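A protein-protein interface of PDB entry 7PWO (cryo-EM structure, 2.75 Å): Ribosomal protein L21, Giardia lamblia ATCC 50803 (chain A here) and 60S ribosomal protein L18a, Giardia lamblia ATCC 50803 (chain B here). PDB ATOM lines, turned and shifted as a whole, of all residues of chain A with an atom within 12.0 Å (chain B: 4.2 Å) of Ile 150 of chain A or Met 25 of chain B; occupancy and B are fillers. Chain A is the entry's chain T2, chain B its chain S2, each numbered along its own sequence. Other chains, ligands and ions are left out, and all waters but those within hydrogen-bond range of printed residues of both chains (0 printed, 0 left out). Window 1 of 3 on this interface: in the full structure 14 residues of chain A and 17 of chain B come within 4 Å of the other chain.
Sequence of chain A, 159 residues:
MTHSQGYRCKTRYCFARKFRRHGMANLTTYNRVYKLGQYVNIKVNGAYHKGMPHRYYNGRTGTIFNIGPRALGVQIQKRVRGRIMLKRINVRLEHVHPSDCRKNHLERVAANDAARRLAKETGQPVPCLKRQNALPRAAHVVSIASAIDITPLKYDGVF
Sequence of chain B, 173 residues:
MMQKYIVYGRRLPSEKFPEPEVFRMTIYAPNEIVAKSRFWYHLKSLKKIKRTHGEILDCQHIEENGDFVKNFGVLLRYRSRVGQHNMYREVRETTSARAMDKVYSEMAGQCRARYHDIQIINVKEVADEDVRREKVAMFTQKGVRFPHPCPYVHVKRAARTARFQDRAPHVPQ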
ATOM      1  N   ILE A 144       1.697  -8.461   1.084  1.00  0.00           N
ATOM      2  CA  ILE A 144       2.168  -7.419   1.992  1.00  0.00           C
ATOM      3  C   ILE A 144       1.004  -6.581   2.496  1.00  0.00           C
ATOM      4  O   ILE A 144       1.169  -5.408   2.844  1.00  0.00           O
ATOM      5  CB  ILE A 144       3.234  -6.542   1.317  1.00  0.00           C
ATOM      6  CG1 ILE A 144       2.638  -5.838   0.090  1.00  0.00           C
ATOM      7  CG2 ILE A 144       4.466  -7.361   1.003  1.00  0.00           C
ATOM      8  CD1 ILE A 144       3.515  -4.794  -0.515  1.00  0.00           C
ATOM      9  N   SER A 146      -0.367  -6.627   5.283  1.00  0.00           N
ATOM     10  CA  SER A 146      -0.329  -6.409   6.730  1.00  0.00           C
ATOM     11  C   SER A 146       1.088  -6.127   7.230  1.00  0.00           C
ATOM     12  O   SER A 146       1.568  -6.739   8.185  1.00  0.00           O
ATOM     13  CB  SER A 146      -0.935  -7.598   7.464  1.00  0.00           C
ATOM     14  OG  SER A 146      -0.818  -7.437   8.861  1.00  0.00           O
ATOM     15  N   ALA A 147       1.780  -5.192   6.595  1.00  0.00           N
ATOM     16  CA  ALA A 147       3.145  -4.871   6.983  1.00  0.00           C
ATOM     17  C   ALA A 147       3.214  -4.260   8.383  1.00  0.00           C
ATOM     18  O   ALA A 147       2.296  -3.567   8.834  1.00  0.00           O
ATOM     19  CB  ALA A 147       3.763  -3.912   5.975  1.00  0.00           C
ATOM     20  N   ILE A 148       4.321  -4.537   9.069  1.00  0.00           N
ATOM     21  CA  ILE A 148       4.665  -3.936  10.356  1.00  0.00           C
ATOM     22  C   ILE A 148       5.848  -3.010  10.127  1.00  0.00           C
ATOM     23  O   ILE A 148       6.843  -3.414   9.517  1.00  0.00           O
ATOM     24  CB  ILE A 148       5.021  -5.005  11.406  1.00  0.00           C
ATOM     25  CG1 ILE A 148       4.102  -6.215  11.274  1.00  0.00           C
ATOM     26  CG2 ILE A 148       4.994  -4.428  12.819  1.00  0.00           C
ATOM     27  CD1 ILE A 148       4.523  -7.379  12.125  1.00  0.00           C
ATOM     28  N   ASP A 149       5.743  -1.774  10.597  1.00  0.00           N
ATOM     29  CA  ASP A 149       6.761  -0.761  10.346  1.00  0.00           C
ATOM     30  C   ASP A 149       7.559  -0.522  11.610  1.00  0.00           C
ATOM     31  O   ASP A 149       7.001  -0.104  12.629  1.00  0.00           O
ATOM     32  CB  ASP A 149       6.140   0.542   9.848  1.00  0.00           C
ATOM     33  CG  ASP A 149       5.696   0.448   8.407  1.00  0.00           C
ATOM     34  OD1 ASP A 149       5.281  -0.656   8.003  1.00  0.00           O
ATOM     35  OD2 ASP A 149       5.779   1.462   7.682  1.00  0.00           O
ATOM     36  N   ILE A 150       8.865  -0.760  11.533  1.00  0.00           N
ATOM     37  CA  ILE A 150       9.745  -0.615  12.678  1.00  0.00           C
ATOM     38  C   ILE A 150      10.850   0.375  12.347  1.00  0.00           C
ATOM     39  O   ILE A 150      11.107   0.701  11.189  1.00  0.00           O
ATOM     40  CB  ILE A 150      10.331  -1.963  13.134  1.00  0.00           C
ATOM     41  CG1 ILE A 150      11.186  -2.584  12.037  1.00  0.00           C
ATOM     42  CG2 ILE A 150       9.220  -2.905  13.545  1.00  0.00           C
ATOM     43  CD1 ILE A 150      11.963  -3.781  12.516  1.00  0.00           C
ATOM     44  N   THR A 151      11.490   0.867  13.399  1.00  0.00           N
ATOM     45  CA  THR A 151      12.512   1.898  13.321  1.00  0.00           C
ATOM     46  C   THR A 151      13.480   1.687  14.471  1.00  0.00           C
ATOM     47  O   THR A 151      13.121   1.071  15.482  1.00  0.00           O
ATOM     48  CB  THR A 151      11.903   3.306  13.403  1.00  0.00           C
ATOM     49  OG1 THR A 151      10.914   3.356  14.442  1.00  0.00           O
ATOM     50  CG2 THR A 151      11.291   3.726  12.071  1.00  0.00           C
ATOM     51  N   PRO A 152      14.704   2.197  14.361  1.00  0.00           N
ATOM     52  CA  PRO A 152      15.608   2.181  15.514  1.00  0.00           C
ATOM     53  C   PRO A 152      14.980   2.900  16.698  1.00  0.00           C
ATOM     54  O   PRO A 152      14.233   3.865  16.540  1.00  0.00           O
ATOM     55  CB  PRO A 152      16.840   2.930  15.004  1.00  0.00           C
ATOM     56  CG  PRO A 152      16.785   2.773  13.519  1.00  0.00           C
ATOM     57  CD  PRO A 152      15.359   2.700  13.144  1.00  0.00           C
ATOM     58  N   LEU A 153      15.270   2.407  17.894  1.00  0.00           N
ATOM     59  CA  LEU A 153      14.791   3.064  19.098  1.00  0.00           C
ATOM     60  C   LEU A 153      15.847   4.001  19.663  1.00  0.00           C
ATOM     61  O   LEU A 153      16.962   4.120  19.151  1.00  0.00           O
ATOM     62  CB  LEU A 153      14.354   2.051  20.159  1.00  0.00           C
ATOM     63  CG  LEU A 153      12.997   1.345  20.040  1.00  0.00           C
ATOM     64  CD1 LEU A 153      12.942   0.319  18.935  1.00  0.00           C
ATOM     65  CD2 LEU A 153      12.619   0.727  21.378  1.00  0.00           C
ATOM     66  N   LYS A 154      15.462   4.690  20.725  1.00  0.00           N
ATOM     67  CA  LYS A 154      16.325   5.635  21.404  1.00  0.00           C
ATOM     68  C   LYS A 154      17.159   4.932  22.465  1.00  0.00           C
ATOM     69  O   LYS A 154      16.736   3.937  23.054  1.00  0.00           O
ATOM     70  CB  LYS A 154      15.490   6.743  22.035  1.00  0.00           C
ATOM     71  CG  LYS A 154      14.511   6.248  23.067  1.00  0.00           C
ATOM     72  CD  LYS A 154      13.678   7.380  23.603  1.00  0.00           C
ATOM     73  CE  LYS A 154      14.529   8.417  24.294  1.00  0.00           C
ATOM     74  NZ  LYS A 154      13.712   9.193  25.253  1.00  0.00           N
ATOM     75  N   TYR B   5      15.359   4.746   0.074  1.00  0.00           N
ATOM     76  CA  TYR B   5      14.931   3.400  -0.260  1.00  0.00           C
ATOM     77  C   TYR B   5      13.910   2.931   0.770  1.00  0.00           C
ATOM     78  O   TYR B   5      14.015   3.266   1.948  1.00  0.00           O
ATOM     79  CB  TYR B   5      16.115   2.419  -0.289  1.00  0.00           C
ATOM     80  CG  TYR B   5      17.205   2.718  -1.297  1.00  0.00           C
ATOM     81  CD1 TYR B   5      18.258   3.570  -0.986  1.00  0.00           C
ATOM     82  CD2 TYR B   5      17.154   2.189  -2.566  1.00  0.00           C
ATOM     83  CE1 TYR B   5      19.243   3.836  -1.900  1.00  0.00           C
ATOM     84  CE2 TYR B   5      18.127   2.451  -3.481  1.00  0.00           C
ATOM     85  CZ  TYR B   5      19.167   3.277  -3.154  1.00  0.00           C
ATOM     86  OH  TYR B   5      20.135   3.543  -4.099  1.00  0.00           O
ATOM     87  N   ILE B   6      12.908   2.181   0.330  1.00  0.00           N
ATOM     88  CA  ILE B   6      12.052   1.408   1.227  1.00  0.00           C
ATOM     89  C   ILE B   6      12.369  -0.061   1.036  1.00  0.00           C
ATOM     90  O   ILE B   6      12.314  -0.572  -0.086  1.00  0.00           O
ATOM     91  CB  ILE B   6      10.549   1.655   1.005  1.00  0.00           C
ATOM     92  CG1 ILE B   6      10.179   3.118   1.187  1.00  0.00           C
ATOM     93  CG2 ILE B   6       9.704   0.785   1.906  1.00  0.00           C
ATOM     94  CD1 ILE B   6       9.033   3.519   0.321  1.00  0.00           C
ATOM     95  N   VAL B   7      12.671  -0.753   2.126  1.00  0.00           N
ATOM     96  CA  VAL B   7      13.059  -2.152   2.044  1.00  0.00           C
ATOM     97  C   VAL B   7      12.028  -2.983   2.793  1.00  0.00           C
ATOM     98  O   VAL B   7      11.696  -2.677   3.946  1.00  0.00           O
ATOM     99  CB  VAL B   7      14.469  -2.390   2.603  1.00  0.00           C
ATOM    100  CG1 VAL B   7      14.786  -3.853   2.577  1.00  0.00           C
ATOM    101  CG2 VAL B   7      15.484  -1.604   1.834  1.00  0.00           C
ATOM    102  N   ARG B  24       8.909  -3.501   6.949  1.00  0.00           N
ATOM    103  CA  ARG B  24       9.408  -2.515   6.007  1.00  0.00           C
ATOM    104  C   ARG B  24      10.056  -1.370   6.767  1.00  0.00           C
ATOM    105  O   ARG B  24       9.667  -1.046   7.892  1.00  0.00           O
ATOM    106  CB  ARG B  24       8.301  -1.989   5.087  1.00  0.00           C
ATOM    107  CG  ARG B  24       7.436  -0.916   5.679  1.00  0.00           C
ATOM    108  CD  ARG B  24       6.865  -0.039   4.599  1.00  0.00           C
ATOM    109  NE  ARG B  24       5.677  -0.640   4.002  1.00  0.00           N
ATOM    110  CZ  ARG B  24       4.460  -0.594   4.531  1.00  0.00           C
ATOM    111  NH1 ARG B  24       4.250   0.031   5.681  1.00  0.00           N
ATOM    112  NH2 ARG B  24       3.445  -1.180   3.910  1.00  0.00           N
ATOM    113  N   MET B  25      11.077  -0.786   6.148  1.00  0.00           N
ATOM    114  CA  MET B  25      11.791   0.335   6.740  1.00  0.00           C
ATOM    115  C   MET B  25      12.204   1.310   5.653  1.00  0.00           C
ATOM    116  O   MET B  25      12.447   0.928   4.507  1.00  0.00           O
ATOM    117  CB  MET B  25      13.043  -0.113   7.529  1.00  0.00           C
ATOM    118  CG  MET B  25      12.735  -0.935   8.786  1.00  0.00           C
ATOM    119  SD  MET B  25      14.148  -1.561   9.720  1.00  0.00           S
ATOM    120  CE  MET B  25      14.812  -0.064  10.441  1.00  0.00           C
ATOM    121  N   THR B  26      12.292   2.578   6.033  1.00  0.00           N
ATOM    122  CA  THR B  26      12.854   3.606   5.175  1.00  0.00           C
ATOM    123  C   THR B  26      14.335   3.768   5.501  1.00  0.00           C
ATOM    124  O   THR B  26      14.703   3.920   6.667  1.00  0.00           O
ATOM    125  CB  THR B  26      12.109   4.928   5.359  1.00  0.00           C
ATOM    126  OG1 THR B  26      10.703   4.674   5.424  1.00  0.00           O
ATOM    127  CG2 THR B  26      12.378   5.868   4.192  1.00  0.00           C
ATOM    128  N   ILE B  27      15.177   3.716   4.470  1.00  0.00           N
ATOM    129  CA  ILE B  27      16.628   3.738   4.596  1.00  0.00           C
ATOM    130  C   ILE B  27      17.163   4.887   3.753  1.00  0.00           C
ATOM    131  O   ILE B  27      16.689   5.121   2.638  1.00  0.00           O
ATOM    132  CB  ILE B  27      17.259   2.399   4.149  1.00  0.00           C
ATOM    133  CG1 ILE B  27      16.723   1.225   4.972  1.00  0.00           C
ATOM    134  CG2 ILE B  27      18.768   2.440   4.265  1.00  0.00           C
ATOM    135  CD1 ILE B  27      17.005   1.315   6.419  1.00  0.00           C
ATOM    136  N   PHE B  39      19.445  -2.422   6.450  1.00  0.00           N
ATOM    137  CA  PHE B  39      18.196  -3.090   6.808  1.00  0.00           C
ATOM    138  C   PHE B  39      18.463  -4.362   7.594  1.00  0.00           C
ATOM    139  O   PHE B  39      17.769  -4.645   8.579  1.00  0.00           O
ATOM    140  CB  PHE B  39      17.371  -3.384   5.550  1.00  0.00           C
ATOM    141  CG  PHE B  39      16.092  -4.155   5.808  1.00  0.00           C
ATOM    142  CD1 PHE B  39      16.108  -5.534   6.001  1.00  0.00           C
ATOM    143  CD2 PHE B  39      14.882  -3.495   5.915  1.00  0.00           C
ATOM    144  CE1 PHE B  39      14.946  -6.228   6.247  1.00  0.00           C
ATOM    145  CE2 PHE B  39      13.714  -4.193   6.169  1.00  0.00           C
ATOM    146  CZ  PHE B  39      13.748  -5.557   6.331  1.00  0.00           C
ATOM    147  N   HIS B  42      19.448  -3.561  11.232  1.00  0.00           N
ATOM    148  CA  HIS B  42      18.361  -3.221  12.148  1.00  0.00           C
ATOM    149  C   HIS B  42      17.451  -4.411  12.425  1.00  0.00           C
ATOM    150  O   HIS B  42      17.054  -4.631  13.574  1.00  0.00           O
ATOM    151  CB  HIS B  42      17.546  -2.051  11.611  1.00  0.00           C
ATOM    152  CG  HIS B  42      18.288  -0.756  11.609  1.00  0.00           C
ATOM    153  ND1 HIS B  42      18.887  -0.243  12.738  1.00  0.00           N
ATOM    154  CD2 HIS B  42      18.548   0.122  10.615  1.00  0.00           C
ATOM    155  CE1 HIS B  42      19.482   0.896  12.439  1.00  0.00           C
ATOM    156  NE2 HIS B  42      19.285   1.143  11.159  1.00  0.00           N
ATOM    157  N   LYS B  47      14.539  -7.624  15.616  1.00  0.00           N
ATOM    158  CA  LYS B  47      13.651  -8.771  15.517  1.00  0.00           C
ATOM    159  C   LYS B  47      14.404 -10.093  15.510  1.00  0.00           C
ATOM    160  O   LYS B  47      13.801 -11.135  15.251  1.00  0.00           O
ATOM    161  CB  LYS B  47      12.763  -8.637  14.287  1.00  0.00           C
ATOM    162  CG  LYS B  47      11.811  -7.447  14.366  1.00  0.00           C
ATOM    163  CD  LYS B  47      10.581  -7.787  15.188  1.00  0.00           C
ATOM    164  CE  LYS B  47       9.840  -6.543  15.629  1.00  0.00           C
ATOM    165  NZ  LYS B  47       8.679  -6.876  16.492  1.00  0.00           N
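The backbone carbonyl oxygen (O) of Ile 148 of chain A lies within hydrogen-bond range of the backbone NH (N) of Arg 24 of chain B, at 3.3 Å. The side-chain carboxylate of Asp 149 of chain A is in salt-bridge range of the guanidinium group of Arg 24 of chain B (2.6 Å).
The backbone NH of Val 7 of chain B is in hydrogen-bond range of the backbone carbonyl oxygen of Met 25 of chain B.
Arg 24 of chain B touches Ala 147 of chain A (NH2 to CB, 3.4 Å). N of Ile 150 of chain A touches O of Arg 24 of chain B (3.7 Å). O of Ile 150 of chain A touches CG of Met 25 of chain B (3.3 Å). Pro 152 of chain A touches Met 25 of chain B. Pro 152 of chain A touches His 42 of chain B.
Ile 150 of chain A touches just these residues of chain B: Arg 24 (3.7 Å) and Met 25 (3.3 Å). Met 25 of chain B touches just these residues of chain A: Ile 150 and Pro 152. No residue of chain A comes within 4 Å of Ile 6 of chain B. No residue of chain A comes within 4 Å of Val 7 of chain B. Printed residues of chain B within 4 Å of Pro 152 of chain A: Met 25 (3.9 Å) and His 42 (3.5 Å). Of the printed residues of chain B, Ile 148 of chain A touches Arg 24 (3.3 Å). Printed residues of chain B within 4 Å of Asp 149 of chain A: Arg 24 (2.6 Å). Printed residues of chain B within 4 Å of Ala 147 of chain A: Arg 24 (3.4 Å). Printed residues of chain A within 4 Å of Arg 24 of chain B: Ala 147, Ile 148, Asp 149 and Ile 150. The nearest residue of chain B that does not touch Ile 150 of chain A is Lys 47 of chain B (4.1 Å). The nearest residue of chain A that does not touch Met 25 of chain B is Thr 151 of chain A (4.2 Å). The nearest printed residue of chain B that does not touch Ile 148 of chain A is Lys 47 of chain B (5.8 Å).
Of the 10 printed residues of chain B, 3 touch a printed residue of chain A. Printed residues of chain B that touch a printed residue of chain A: Arg 24, Met 25 and His 42. Hydrophobic or aromatic side chains of chain B within 4 Å of the printed part of chain A: Met 25 and His 42. Hydrophobic or aromatic side chains of chain A that line the printed part of chain B: Ala 147, Ile 150 and Pro 152.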
